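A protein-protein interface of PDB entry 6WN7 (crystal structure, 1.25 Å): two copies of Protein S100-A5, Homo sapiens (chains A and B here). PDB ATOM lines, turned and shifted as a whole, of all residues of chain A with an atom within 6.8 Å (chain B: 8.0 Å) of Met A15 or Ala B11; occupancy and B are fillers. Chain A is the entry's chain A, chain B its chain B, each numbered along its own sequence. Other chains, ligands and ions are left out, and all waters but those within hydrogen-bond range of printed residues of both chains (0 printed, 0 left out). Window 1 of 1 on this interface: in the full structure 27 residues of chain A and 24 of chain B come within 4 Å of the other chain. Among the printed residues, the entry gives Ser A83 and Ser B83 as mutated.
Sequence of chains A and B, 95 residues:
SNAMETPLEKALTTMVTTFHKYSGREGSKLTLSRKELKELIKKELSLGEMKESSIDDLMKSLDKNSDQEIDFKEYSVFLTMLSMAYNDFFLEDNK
A ring nitrogen (NE2) of His A20 is in hydrogen-bond range of the side-chain amide oxygen (OD1) of Asn B87, 2.5 Å away.
O of Thr A13 sits close to OG1 of Thr A17, 3.4 Å away. The backbone carbonyl oxygen (O) of Thr A14 lies within hydrogen-bond range of the side-chain hydroxyl (OG1) of Thr A17 (3.5 Å). The side-chain hydroxyl (OG1) of Thr A18 lies within hydrogen-bond range of the backbone carbonyl oxygen (O) of Thr A14 (2.5 Å). OH of Tyr A75 is in hydrogen-bond range of O of Met A15. O of Lys B10 lies within hydrogen-bond range of OG1 of Thr B14 (3.1 Å). The side-chain hydroxyl of Thr B18 is in hydrogen-bond range of the backbone carbonyl oxygen of Thr B14 (3.0 Å).
CG2 of Thr B14 touches O of Pro A7, at 3.8 Å. Met B15 touches Leu A8 (CE to CD1, 3.1 Å). O of Ala A11 touches CB of Ala B11, 3.6 Å away. CD2 of Leu A12 touches OG of Ser B83, 3.3 Å away. Thr A14 touches Pro B7 (CG2 to C, 3.8 Å). Leu B8 touches Thr A14 (N to CG2, 3.8 Å). Met B15 touches Met A15 (CE to CE, 3.1 Å). OD1 of Asn B87 touches CG1 of Val A16, 3.4 Å away. O of Leu A79 touches CD2 of Leu B12 (3.8 Å). Ser A83 touches Val B16 (O to CG2, 3.6 Å).
Of the printed residues of chain B, Ala A11 touches Ala B11, Thr B14 and Met B15. Of the printed residues of chain B, Leu A12 touches Leu B79 (3.8 Å) and Ser B83 (3.3 Å). Of the printed residues of chain B, Thr A13 touches Tyr B86. Printed residues of chain B within 4 Å of Thr A14: Pro B7 and Leu B8. Printed residues of chain B within 4 Å of Met A15: Ala B11 (3.9 Å) and Met B15 (3.1 Å). Printed residues of chain B within 4 Å of Ser A83: Leu B12 (3.5 Å) and Val B16 (3.6 Å). Thr B6 touches none of the printed residues of chain A. Of the printed residues of chain A, Ala B11 touches Ala A11 (3.6 Å) and Met A15 (3.9 Å). The nearest printed residue of chain A that does not touch Ala B11 is Thr A14 (4.3 Å). The nearest printed residue of chain B that does not touch Thr A13 is Ser B83 (6.6 Å).
Hydrophobic or aromatic side chains of chain B within 4 Å of the printed part of chain A: Pro B7, Leu B8, Ala B11, Leu B12, Met B15, Val B16 and Tyr B86. Of the 18 printed residues of chain A, 14 touch a printed residue of chain B. Along chain A the printed residues that touch a printed residue of chain B span positions 7 to 83.
Ala B11 touches its own counterpart, Ala A11. Ala A11 touches Met B15, and with the chains exchanged Met A15 touches Ala B11. Val A16 touches Ser B83, and with the chains exchanged Ser A83 touches Val B16. Thr A18 touches Leu B8, but with the chains exchanged Leu A8 does not touch Thr B18 (4.5 Å).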
ATOM      1  N   PRO A   7      27.849  14.242 -22.711  1.00  0.00           N
ATOM      2  CA  PRO A   7      26.585  13.987 -21.996  1.00  0.00           C
ATOM      3  C   PRO A   7      25.535  15.050 -22.236  1.00  0.00           C
ATOM      4  O   PRO A   7      24.349  14.734 -22.298  1.00  0.00           O
ATOM      5  CB  PRO A   7      27.010  13.956 -20.518  1.00  0.00           C
ATOM      6  CG  PRO A   7      28.440  13.672 -20.539  1.00  0.00           C
ATOM      7  CD  PRO A   7      29.007  14.239 -21.802  1.00  0.00           C
ATOM      8  N   LEU A   8      25.948  16.309 -22.344  1.00  0.00           N
ATOM      9  CA  LEU A   8      25.007  17.387 -22.599  1.00  0.00           C
ATOM     10  C   LEU A   8      24.481  17.327 -24.026  1.00  0.00           C
ATOM     11  O   LEU A   8      23.302  17.591 -24.282  1.00  0.00           O
ATOM     12  CB  LEU A   8      25.691  18.720 -22.355  1.00  0.00           C
ATOM     13  CG  LEU A   8      24.807  19.919 -22.639  1.00  0.00           C
ATOM     14  CD1 LEU A   8      23.729  20.063 -21.584  1.00  0.00           C
ATOM     15  CD2 LEU A   8      25.680  21.171 -22.750  1.00  0.00           C
ATOM     16  N   LYS A  10      24.119  14.621 -25.874  1.00  0.00           N
ATOM     17  CA  LYS A  10      23.143  13.541 -25.947  1.00  0.00           C
ATOM     18  C   LYS A  10      21.823  13.963 -25.321  1.00  0.00           C
ATOM     19  O   LYS A  10      20.756  13.716 -25.882  1.00  0.00           O
ATOM     20  CB  LYS A  10      23.716  12.268 -25.333  1.00  0.00           C
ATOM     21  CG  LYS A  10      24.903  11.738 -26.140  1.00  0.00           C
ATOM     22  CD  LYS A  10      25.308  10.313 -25.775  1.00  0.00           C
ATOM     23  CE  LYS A  10      25.718   9.489 -26.994  1.00  0.00           C
ATOM     24  NZ  LYS A  10      25.602   8.026 -26.737  1.00  0.00           N
ATOM     25  N   ALA A  11      21.888  14.649 -24.189  1.00  0.00           N
ATOM     26  CA  ALA A  11      20.681  15.157 -23.561  1.00  0.00           C
ATOM     27  C   ALA A  11      19.891  16.030 -24.510  1.00  0.00           C
ATOM     28  O   ALA A  11      18.691  15.830 -24.696  1.00  0.00           O
ATOM     29  CB  ALA A  11      21.068  15.975 -22.335  1.00  0.00           C
ATOM     30  N   LEU A  12      20.533  17.042 -25.081  1.00  0.00           N
ATOM     31  CA  LEU A  12      19.833  17.953 -25.985  1.00  0.00           C
ATOM     32  C   LEU A  12      19.283  17.217 -27.195  1.00  0.00           C
ATOM     33  O   LEU A  12      18.245  17.590 -27.722  1.00  0.00           O
ATOM     34  CB  LEU A  12      20.772  19.070 -26.431  1.00  0.00           C
ATOM     35  CG  LEU A  12      21.213  20.024 -25.321  1.00  0.00           C
ATOM     36  CD1 LEU A  12      22.460  20.739 -25.654  1.00  0.00           C
ATOM     37  CD2 LEU A  12      20.119  21.032 -25.063  1.00  0.00           C
ATOM     38  N   THR A  13      19.968  16.177 -27.647  1.00  0.00           N
ATOM     39  CA  THR A  13      19.477  15.388 -28.766  1.00  0.00           C
ATOM     40  C   THR A  13      18.204  14.653 -28.376  1.00  0.00           C
ATOM     41  O   THR A  13      17.244  14.575 -29.150  1.00  0.00           O
ATOM     42  CB  THR A  13      20.566  14.397 -29.157  1.00  0.00           C
ATOM     43  OG1 THR A  13      21.711  15.106 -29.640  1.00  0.00           O
ATOM     44  CG2 THR A  13      20.081  13.472 -30.224  1.00  0.00           C
ATOM     45  N   THR A  14      18.174  14.127 -27.163  1.00  0.00           N
ATOM     46  CA  THR A  14      16.994  13.423 -26.689  1.00  0.00           C
ATOM     47  C   THR A  14      15.815  14.363 -26.546  1.00  0.00           C
ATOM     48  O   THR A  14      14.681  13.990 -26.846  1.00  0.00           O
ATOM     49  CB  THR A  14      17.324  12.764 -25.360  1.00  0.00           C
ATOM     50  OG1 THR A  14      18.349  11.795 -25.589  1.00  0.00           O
ATOM     51  CG2 THR A  14      16.087  12.139 -24.775  1.00  0.00           C
ATOM     52  N   MET A  15      16.056  15.580 -26.072  1.00  0.00           N
ATOM     53  CA  MET A  15      14.976  16.554 -26.012  1.00  0.00           C
ATOM     54  C   MET A  15      14.361  16.761 -27.385  1.00  0.00           C
ATOM     55  O   MET A  15      13.135  16.857 -27.517  1.00  0.00           O
ATOM     56  CB  MET A  15      15.498  17.878 -25.476  1.00  0.00           C
ATOM     57  CG  MET A  15      15.943  17.795 -24.035  1.00  0.00           C
ATOM     58  SD  MET A  15      16.919  19.225 -23.561  1.00  0.00           S
ATOM     59  CE  MET A  15      18.266  18.444 -22.736  1.00  0.00           C
ATOM     60  N   VAL A  16      15.198  16.816 -28.421  1.00  0.00           N
ATOM     61  CA  VAL A  16      14.694  17.078 -29.768  1.00  0.00           C
ATOM     62  C   VAL A  16      13.979  15.856 -30.340  1.00  0.00           C
ATOM     63  O   VAL A  16      12.895  15.981 -30.927  1.00  0.00           O
ATOM     64  CB  VAL A  16      15.816  17.562 -30.711  1.00  0.00           C
ATOM     65  CG1 VAL A  16      15.273  17.692 -32.131  1.00  0.00           C
ATOM     66  CG2 VAL A  16      16.380  18.886 -30.298  1.00  0.00           C
ATOM     67  N   THR A  17      14.573  14.658 -30.213  1.00  0.00           N
ATOM     68  CA  THR A  17      13.938  13.476 -30.806  1.00  0.00           C
ATOM     69  C   THR A  17      12.624  13.126 -30.111  1.00  0.00           C
ATOM     70  O   THR A  17      11.680  12.670 -30.761  1.00  0.00           O
ATOM     71  CB  THR A  17      14.907  12.298 -30.850  1.00  0.00           C
ATOM     72  OG1 THR A  17      15.236  11.862 -29.537  1.00  0.00           O
ATOM     73  CG2 THR A  17      16.191  12.701 -31.541  1.00  0.00           C
ATOM     74  N   THR A  18      12.528  13.371 -28.805  1.00  0.00           N
ATOM     75  CA  THR A  18      11.301  13.077 -28.066  1.00  0.00           C
ATOM     76  C   THR A  18      10.111  13.880 -28.589  1.00  0.00           C
ATOM     77  O   THR A  18       8.995  13.363 -28.671  1.00  0.00           O
ATOM     78  CB  THR A  18      11.548  13.347 -26.582  1.00  0.00           C
ATOM     79  OG1 THR A  18      12.682  12.593 -26.157  1.00  0.00           O
ATOM     80  CG2 THR A  18      10.363  12.941 -25.765  1.00  0.00           C
ATOM     81  N   PHE A  19      10.326  15.145 -28.933  1.00  0.00           N
ATOM     82  CA  PHE A  19       9.276  15.959 -29.540  1.00  0.00           C
ATOM     83  C   PHE A  19       8.780  15.333 -30.834  1.00  0.00           C
ATOM     84  O   PHE A  19       7.579  15.130 -31.012  1.00  0.00           O
ATOM     85  CB  PHE A  19       9.822  17.358 -29.816  1.00  0.00           C
ATOM     86  CG  PHE A  19       8.871  18.255 -30.554  1.00  0.00           C
ATOM     87  CD1 PHE A  19       7.961  19.011 -29.874  1.00  0.00           C
ATOM     88  CD2 PHE A  19       8.915  18.370 -31.933  1.00  0.00           C
ATOM     89  CE1 PHE A  19       7.116  19.825 -30.538  1.00  0.00           C
ATOM     90  CE2 PHE A  19       8.060  19.205 -32.598  1.00  0.00           C
ATOM     91  CZ  PHE A  19       7.165  19.922 -31.898  1.00  0.00           C
ATOM     92  N   HIS A  20       9.702  15.024 -31.758  1.00  0.00           N
ATOM     93  CA  HIS A  20       9.306  14.548 -33.074  1.00  0.00           C
ATOM     94  C   HIS A  20       8.745  13.136 -33.023  1.00  0.00           C
ATOM     95  O   HIS A  20       7.952  12.764 -33.888  1.00  0.00           O
ATOM     96  CB  HIS A  20      10.485  14.683 -34.028  1.00  0.00           C
ATOM     97  CG  HIS A  20      10.877  16.105 -34.292  1.00  0.00           C
ATOM     98  ND1 HIS A  20      10.201  16.915 -35.177  1.00  0.00           N
ATOM     99  CD2 HIS A  20      11.868  16.865 -33.776  1.00  0.00           C
ATOM    100  CE1 HIS A  20      10.764  18.107 -35.202  1.00  0.00           C
ATOM    101  NE2 HIS A  20      11.785  18.100 -34.367  1.00  0.00           N
ATOM    102  N   LEU A  40       3.048  12.249 -24.808  1.00  0.00           N
ATOM    103  CA  LEU A  40       4.446  12.425 -24.405  1.00  0.00           C
ATOM    104  C   LEU A  40       4.571  12.602 -22.893  1.00  0.00           C
ATOM    105  O   LEU A  40       5.472  12.041 -22.258  1.00  0.00           O
ATOM    106  CB  LEU A  40       5.035  13.649 -25.118  1.00  0.00           C
ATOM    107  CG  LEU A  40       6.536  13.907 -24.980  1.00  0.00           C
ATOM    108  CD1 LEU A  40       7.006  14.741 -26.177  1.00  0.00           C
ATOM    109  CD2 LEU A  40       6.892  14.598 -23.689  1.00  0.00           C
ATOM    110  N   PHE A  72       7.984  23.298 -31.730  1.00  0.00           N
ATOM    111  CA  PHE A  72       9.235  22.977 -31.013  1.00  0.00           C
ATOM    112  C   PHE A  72       9.607  24.115 -30.010  1.00  0.00           C
ATOM    113  O   PHE A  72      10.070  23.859 -28.901  1.00  0.00           O
ATOM    114  CB  PHE A  72      10.466  22.667 -31.903  1.00  0.00           C
ATOM    115  CG  PHE A  72      11.664  22.248 -31.064  1.00  0.00           C
ATOM    116  CD1 PHE A  72      11.704  20.979 -30.494  1.00  0.00           C
ATOM    117  CD2 PHE A  72      12.685  23.126 -30.773  1.00  0.00           C
ATOM    118  CE1 PHE A  72      12.727  20.608 -29.669  1.00  0.00           C
ATOM    119  CE2 PHE A  72      13.703  22.721 -29.989  1.00  0.00           C
ATOM    120  CZ  PHE A  72      13.721  21.445 -29.454  1.00  0.00           C
ATOM    121  N   TYR A  75       7.444  23.862 -27.020  1.00  0.00           N
ATOM    122  CA  TYR A  75       7.844  22.705 -26.216  1.00  0.00           C
ATOM    123  C   TYR A  75       9.134  22.946 -25.453  1.00  0.00           C
ATOM    124  O   TYR A  75       9.320  22.399 -24.366  1.00  0.00           O
ATOM    125  CB  TYR A  75       7.974  21.507 -27.153  1.00  0.00           C
ATOM    126  CG  TYR A  75       8.809  20.322 -26.726  1.00  0.00           C
ATOM    127  CD1 TYR A  75       8.272  19.305 -25.948  1.00  0.00           C
ATOM    128  CD2 TYR A  75      10.100  20.169 -27.187  1.00  0.00           C
ATOM    129  CE1 TYR A  75       9.024  18.191 -25.598  1.00  0.00           C
ATOM    130  CE2 TYR A  75      10.854  19.069 -26.856  1.00  0.00           C
ATOM    131  CZ  TYR A  75      10.320  18.069 -26.060  1.00  0.00           C
ATOM    132  OH  TYR A  75      11.107  16.962 -25.749  1.00  0.00           O
ATOM    133  N   LEU A  79       9.920  22.228 -21.447  1.00  0.00           N
ATOM    134  CA  LEU A  79      11.080  21.526 -20.910  1.00  0.00           C
ATOM    135  C   LEU A  79      11.798  22.368 -19.865  1.00  0.00           C
ATOM    136  O   LEU A  79      12.178  21.855 -18.819  1.00  0.00           O
ATOM    137  CB  LEU A  79      12.029  21.154 -22.047  1.00  0.00           C
ATOM    138  CG  LEU A  79      11.583  20.086 -23.041  1.00  0.00           C
ATOM    139  CD1 LEU A  79      12.772  19.749 -23.907  1.00  0.00           C
ATOM    140  CD2 LEU A  79      11.066  18.858 -22.372  1.00  0.00           C
ATOM    141  N   SER A  83      12.766  21.612 -15.944  1.00  0.00           N
ATOM    142  CA  SER A  83      14.149  21.709 -15.495  1.00  0.00           C
ATOM    143  C   SER A  83      14.267  22.616 -14.289  1.00  0.00           C
ATOM    144  O   SER A  83      14.973  22.300 -13.331  1.00  0.00           O
ATOM    145  CB  SER A  83      15.009  22.278 -16.624  1.00  0.00           C
ATOM    146  OG  SER A  83      15.406  21.263 -17.510  1.00  0.00           O
ATOM    147  N   GLU B   5      14.474   8.474 -15.004  1.00  0.00           N
ATOM    148  CA  GLU B   5      14.405   7.105 -15.487  1.00  0.00           C
ATOM    149  C   GLU B   5      14.114   6.962 -16.978  1.00  0.00           C
ATOM    150  O   GLU B   5      14.691   6.083 -17.595  1.00  0.00           O
ATOM    151  CB  GLU B   5      13.399   6.288 -14.691  1.00  0.00           C
ATOM    152  CG  GLU B   5      13.487   4.807 -14.945  1.00  0.00           C
ATOM    153  CD  GLU B   5      12.528   4.370 -16.032  1.00  0.00           C
ATOM    154  OE1 GLU B   5      12.803   3.367 -16.734  1.00  0.00           O
ATOM    155  OE2 GLU B   5      11.483   5.031 -16.183  1.00  0.00           O
ATOM    156  N   THR B   6      13.235   7.798 -17.559  1.00  0.00           N
ATOM    157  CA  THR B   6      13.132   7.825 -19.015  1.00  0.00           C
ATOM    158  C   THR B   6      14.341   8.555 -19.583  1.00  0.00           C
ATOM    159  O   THR B   6      15.005   9.300 -18.866  1.00  0.00           O
ATOM    160  CB  THR B   6      11.876   8.540 -19.516  1.00  0.00           C
ATOM    161  OG1 THR B   6      11.938   9.934 -19.217  1.00  0.00           O
ATOM    162  CG2 THR B   6      10.641   7.963 -18.899  1.00  0.00           C
ATOM    163  N   PRO B   7      14.635   8.384 -20.878  1.00  0.00           N
ATOM    164  CA  PRO B   7      15.683   9.223 -21.486  1.00  0.00           C
ATOM    165  C   PRO B   7      15.388  10.706 -21.377  1.00  0.00           C
ATOM    166  O   PRO B   7      16.285  11.482 -21.070  1.00  0.00           O
ATOM    167  CB  PRO B   7      15.727   8.751 -22.944  1.00  0.00           C
ATOM    168  CG  PRO B   7      15.030   7.463 -22.951  1.00  0.00           C
ATOM    169  CD  PRO B   7      14.018   7.491 -21.865  1.00  0.00           C
ATOM    170  N   LEU B   8      14.151  11.128 -21.605  1.00  0.00           N
ATOM    171  CA  LEU B   8      13.843  12.545 -21.477  1.00  0.00           C
ATOM    172  C   LEU B   8      14.018  13.028 -20.039  1.00  0.00           C
ATOM    173  O   LEU B   8      14.471  14.156 -19.812  1.00  0.00           O
ATOM    174  CB  LEU B   8      12.438  12.825 -21.987  1.00  0.00           C
ATOM    175  CG  LEU B   8      12.028  14.291 -21.843  1.00  0.00           C
ATOM    176  CD1 LEU B   8      12.958  15.226 -22.627  1.00  0.00           C
ATOM    177  CD2 LEU B   8      10.583  14.429 -22.265  1.00  0.00           C
ATOM    178  N   GLU B   9      13.663  12.193 -19.048  1.00  0.00           N
ATOM    179  CA  GLU B   9      13.837  12.613 -17.666  1.00  0.00           C
ATOM    180  C   GLU B   9      15.305  12.730 -17.319  1.00  0.00           C
ATOM    181  O   GLU B   9      15.714  13.674 -16.646  1.00  0.00           O
ATOM    182  CB  GLU B   9      13.137  11.664 -16.703  1.00  0.00           C
ATOM    183  CG  GLU B   9      11.616  11.751 -16.738  1.00  0.00           C
ATOM    184  CD  GLU B   9      10.945  10.744 -15.825  1.00  0.00           C
ATOM    185  OE1 GLU B   9      10.133  11.167 -15.000  1.00  0.00           O
ATOM    186  OE2 GLU B   9      11.213   9.537 -15.924  1.00  0.00           O
ATOM    187  N   LYS B  10      16.122  11.790 -17.779  1.00  0.00           N
ATOM    188  CA  LYS B  10      17.546  11.889 -17.505  1.00  0.00           C
ATOM    189  C   LYS B  10      18.173  13.069 -18.228  1.00  0.00           C
ATOM    190  O   LYS B  10      19.155  13.638 -17.742  1.00  0.00           O
ATOM    191  CB  LYS B  10      18.243  10.610 -17.931  1.00  0.00           C
ATOM    192  CG  LYS B  10      17.829   9.407 -17.167  1.00  0.00           C
ATOM    193  CD  LYS B  10      18.616   8.228 -17.691  1.00  0.00           C
ATOM    194  CE  LYS B  10      18.110   6.889 -17.145  1.00  0.00           C
ATOM    195  NZ  LYS B  10      18.722   5.720 -17.853  1.00  0.00           N
ATOM    196  N   ALA B  11      17.632  13.432 -19.391  1.00  0.00           N
ATOM    197  CA  ALA B  11      18.137  14.569 -20.155  1.00  0.00           C
ATOM    198  C   ALA B  11      17.920  15.868 -19.404  1.00  0.00           C
ATOM    199  O   ALA B  11      18.825  16.692 -19.309  1.00  0.00           O
ATOM    200  CB  ALA B  11      17.450  14.627 -21.516  1.00  0.00           C
ATOM    201  N   LEU B  12      16.727  16.060 -18.857  1.00  0.00           N
ATOM    202  CA  LEU B  12      16.453  17.264 -18.086  1.00  0.00           C
ATOM    203  C   LEU B  12      17.281  17.308 -16.806  1.00  0.00           C
ATOM    204  O   LEU B  12      17.738  18.382 -16.391  1.00  0.00           O
ATOM    205  CB  LEU B  12      14.964  17.323 -17.779  1.00  0.00           C
ATOM    206  CG  LEU B  12      14.058  17.387 -18.999  1.00  0.00           C
ATOM    207  CD1 LEU B  12      12.651  17.166 -18.571  1.00  0.00           C
ATOM    208  CD2 LEU B  12      14.209  18.724 -19.662  1.00  0.00           C
ATOM    209  N   THR B  13      17.492  16.154 -16.173  1.00  0.00           N
ATOM    210  CA  THR B  13      18.364  16.110 -15.011  1.00  0.00           C
ATOM    211  C   THR B  13      19.775  16.529 -15.384  1.00  0.00           C
ATOM    212  O   THR B  13      20.461  17.192 -14.600  1.00  0.00           O
ATOM    213  CB  THR B  13      18.370  14.710 -14.412  1.00  0.00           C
ATOM    214  OG1 THR B  13      17.063  14.386 -13.974  1.00  0.00           O
ATOM    215  CG2 THR B  13      19.287  14.680 -13.254  1.00  0.00           C
ATOM    216  N   THR B  14      20.226  16.137 -16.578  1.00  0.00           N
ATOM    217  CA  THR B  14      21.562  16.483 -17.041  1.00  0.00           C
ATOM    218  C   THR B  14      21.698  17.982 -17.276  1.00  0.00           C
ATOM    219  O   THR B  14      22.746  18.566 -16.982  1.00  0.00           O
ATOM    220  CB  THR B  14      21.858  15.643 -18.289  1.00  0.00           C
ATOM    221  OG1 THR B  14      22.148  14.294 -17.870  1.00  0.00           O
ATOM    222  CG2 THR B  14      23.000  16.198 -19.120  1.00  0.00           C
ATOM    223  N   MET B  15      20.648  18.630 -17.771  1.00  0.00           N
ATOM    224  CA  MET B  15      20.702  20.075 -17.936  1.00  0.00           C
ATOM    225  C   MET B  15      21.074  20.745 -16.628  1.00  0.00           C
ATOM    226  O   MET B  15      21.839  21.709 -16.611  1.00  0.00           O
ATOM    227  CB  MET B  15      19.333  20.611 -18.371  1.00  0.00           C
ATOM    228  CG  MET B  15      18.832  20.123 -19.694  1.00  0.00           C
ATOM    229  SD  MET B  15      19.951  20.522 -21.029  1.00  0.00           S
ATOM    230  CE  MET B  15      20.841  18.988 -21.112  1.00  0.00           C
ATOM    231  N   VAL B  16      20.516  20.249 -15.522  1.00  0.00           N
ATOM    232  CA  VAL B  16      20.687  20.854 -14.207  1.00  0.00           C
ATOM    233  C   VAL B  16      22.063  20.543 -13.632  1.00  0.00           C
ATOM    234  O   VAL B  16      22.795  21.435 -13.213  1.00  0.00           O
ATOM    235  CB  VAL B  16      19.556  20.375 -13.264  1.00  0.00           C
ATOM    236  CG1 VAL B  16      19.735  20.927 -11.843  1.00  0.00           C
ATOM    237  CG2 VAL B  16      18.173  20.729 -13.857  1.00  0.00           C
ATOM    238  N   THR B  17      22.421  19.268 -13.560  1.00  0.00           N
ATOM    239  CA  THR B  17      23.684  18.910 -12.942  1.00  0.00           C
ATOM    240  C   THR B  17      24.867  19.435 -13.735  1.00  0.00           C
ATOM    241  O   THR B  17      25.897  19.762 -13.142  1.00  0.00           O
ATOM    242  CB  THR B  17      23.770  17.402 -12.754  1.00  0.00           C
ATOM    243  OG1 THR B  17      23.843  16.747 -14.022  1.00  0.00           O
ATOM    244  CG2 THR B  17      22.548  16.897 -12.040  1.00  0.00           C
ATOM    245  N   THR B  18      24.758  19.546 -15.061  1.00  0.00           N
ATOM    246  CA  THR B  18      25.865  20.129 -15.815  1.00  0.00           C
ATOM    247  C   THR B  18      26.090  21.579 -15.405  1.00  0.00           C
ATOM    248  O   THR B  18      27.213  21.971 -15.101  1.00  0.00           O
ATOM    249  CB  THR B  18      25.641  20.013 -17.324  1.00  0.00           C
ATOM    250  OG1 THR B  18      25.658  18.636 -17.735  1.00  0.00           O
ATOM    251  CG2 THR B  18      26.744  20.774 -18.073  1.00  0.00           C
ATOM    252  N   LEU B  79      20.952  26.887 -23.759  1.00  0.00           N
ATOM    253  CA  LEU B  79      20.495  25.537 -24.068  1.00  0.00           C
ATOM    254  C   LEU B  79      19.480  25.544 -25.204  1.00  0.00           C
ATOM    255  O   LEU B  79      19.508  24.679 -26.080  1.00  0.00           O
ATOM    256  CB  LEU B  79      19.878  24.891 -22.824  1.00  0.00           C
ATOM    257  CG  LEU B  79      20.779  24.567 -21.632  1.00  0.00           C
ATOM    258  CD1 LEU B  79      19.959  23.958 -20.513  1.00  0.00           C
ATOM    259  CD2 LEU B  79      21.870  23.638 -22.039  1.00  0.00           C
ATOM    260  N   THR B  80      18.564  26.508 -25.192  1.00  0.00           N
ATOM    261  CA  THR B  80      17.594  26.615 -26.268  1.00  0.00           C
ATOM    262  C   THR B  80      18.261  26.919 -27.608  1.00  0.00           C
ATOM    263  O   THR B  80      17.856  26.377 -28.642  1.00  0.00           O
ATOM    264  CB  THR B  80      16.559  27.673 -25.910  1.00  0.00           C
ATOM    265  OG1 THR B  80      15.971  27.356 -24.649  1.00  0.00           O
ATOM    266  CG2 THR B  80      15.464  27.681 -26.909  1.00  0.00           C
ATOM    267  N   SER B  83      19.510  23.504 -28.645  1.00  0.00           N
ATOM    268  CA  SER B  83      18.391  22.661 -29.056  1.00  0.00           C
ATOM    269  C   SER B  83      17.875  23.092 -30.417  1.00  0.00           C
ATOM    270  O   SER B  83      17.704  22.270 -31.324  1.00  0.00           O
ATOM    271  CB  SER B  83      17.252  22.766 -28.038  1.00  0.00           C
ATOM    272  OG  SER B  83      17.635  22.268 -26.782  1.00  0.00           O
ATOM    273  N   TYR B  86      20.099  21.954 -33.155  1.00  0.00           N
ATOM    274  CA  TYR B  86      19.982  20.548 -33.495  1.00  0.00           C
ATOM    275  C   TYR B  86      18.611  20.249 -34.091  1.00  0.00           C
ATOM    276  O   TYR B  86      18.493  19.397 -34.972  1.00  0.00           O
ATOM    277  CB  TYR B  86      20.297  19.630 -32.326  1.00  0.00           C
ATOM    278  CG  TYR B  86      20.310  18.167 -32.765  1.00  0.00           C
ATOM    279  CD1 TYR B  86      21.372  17.633 -33.470  1.00  0.00           C
ATOM    280  CD2 TYR B  86      19.239  17.336 -32.500  1.00  0.00           C
ATOM    281  CE1 TYR B  86      21.371  16.318 -33.871  1.00  0.00           C
ATOM    282  CE2 TYR B  86      19.234  16.030 -32.910  1.00  0.00           C
ATOM    283  CZ  TYR B  86      20.293  15.528 -33.596  1.00  0.00           C
ATOM    284  OH  TYR B  86      20.266  14.222 -33.999  1.00  0.00           O
ATOM    285  N   ASN B  87      17.570  20.954 -33.656  1.00  0.00           N
ATOM    286  CA  ASN B  87      16.262  20.721 -34.251  1.00  0.00           C
ATOM    287  C   ASN B  87      16.317  20.980 -35.749  1.00  0.00           C
ATOM    288  O   ASN B  87      15.862  20.160 -36.550  1.00  0.00           O
ATOM    289  CB  ASN B  87      15.192  21.577 -33.578  1.00  0.00           C
ATOM    290  CG  ASN B  87      13.775  21.137 -33.954  1.00  0.00           C
ATOM    291  OD1 ASN B  87      13.407  19.972 -33.798  1.00  0.00           O
ATOM    292  ND2 ASN B  87      12.983  22.078 -34.473  1.00  0.00           N
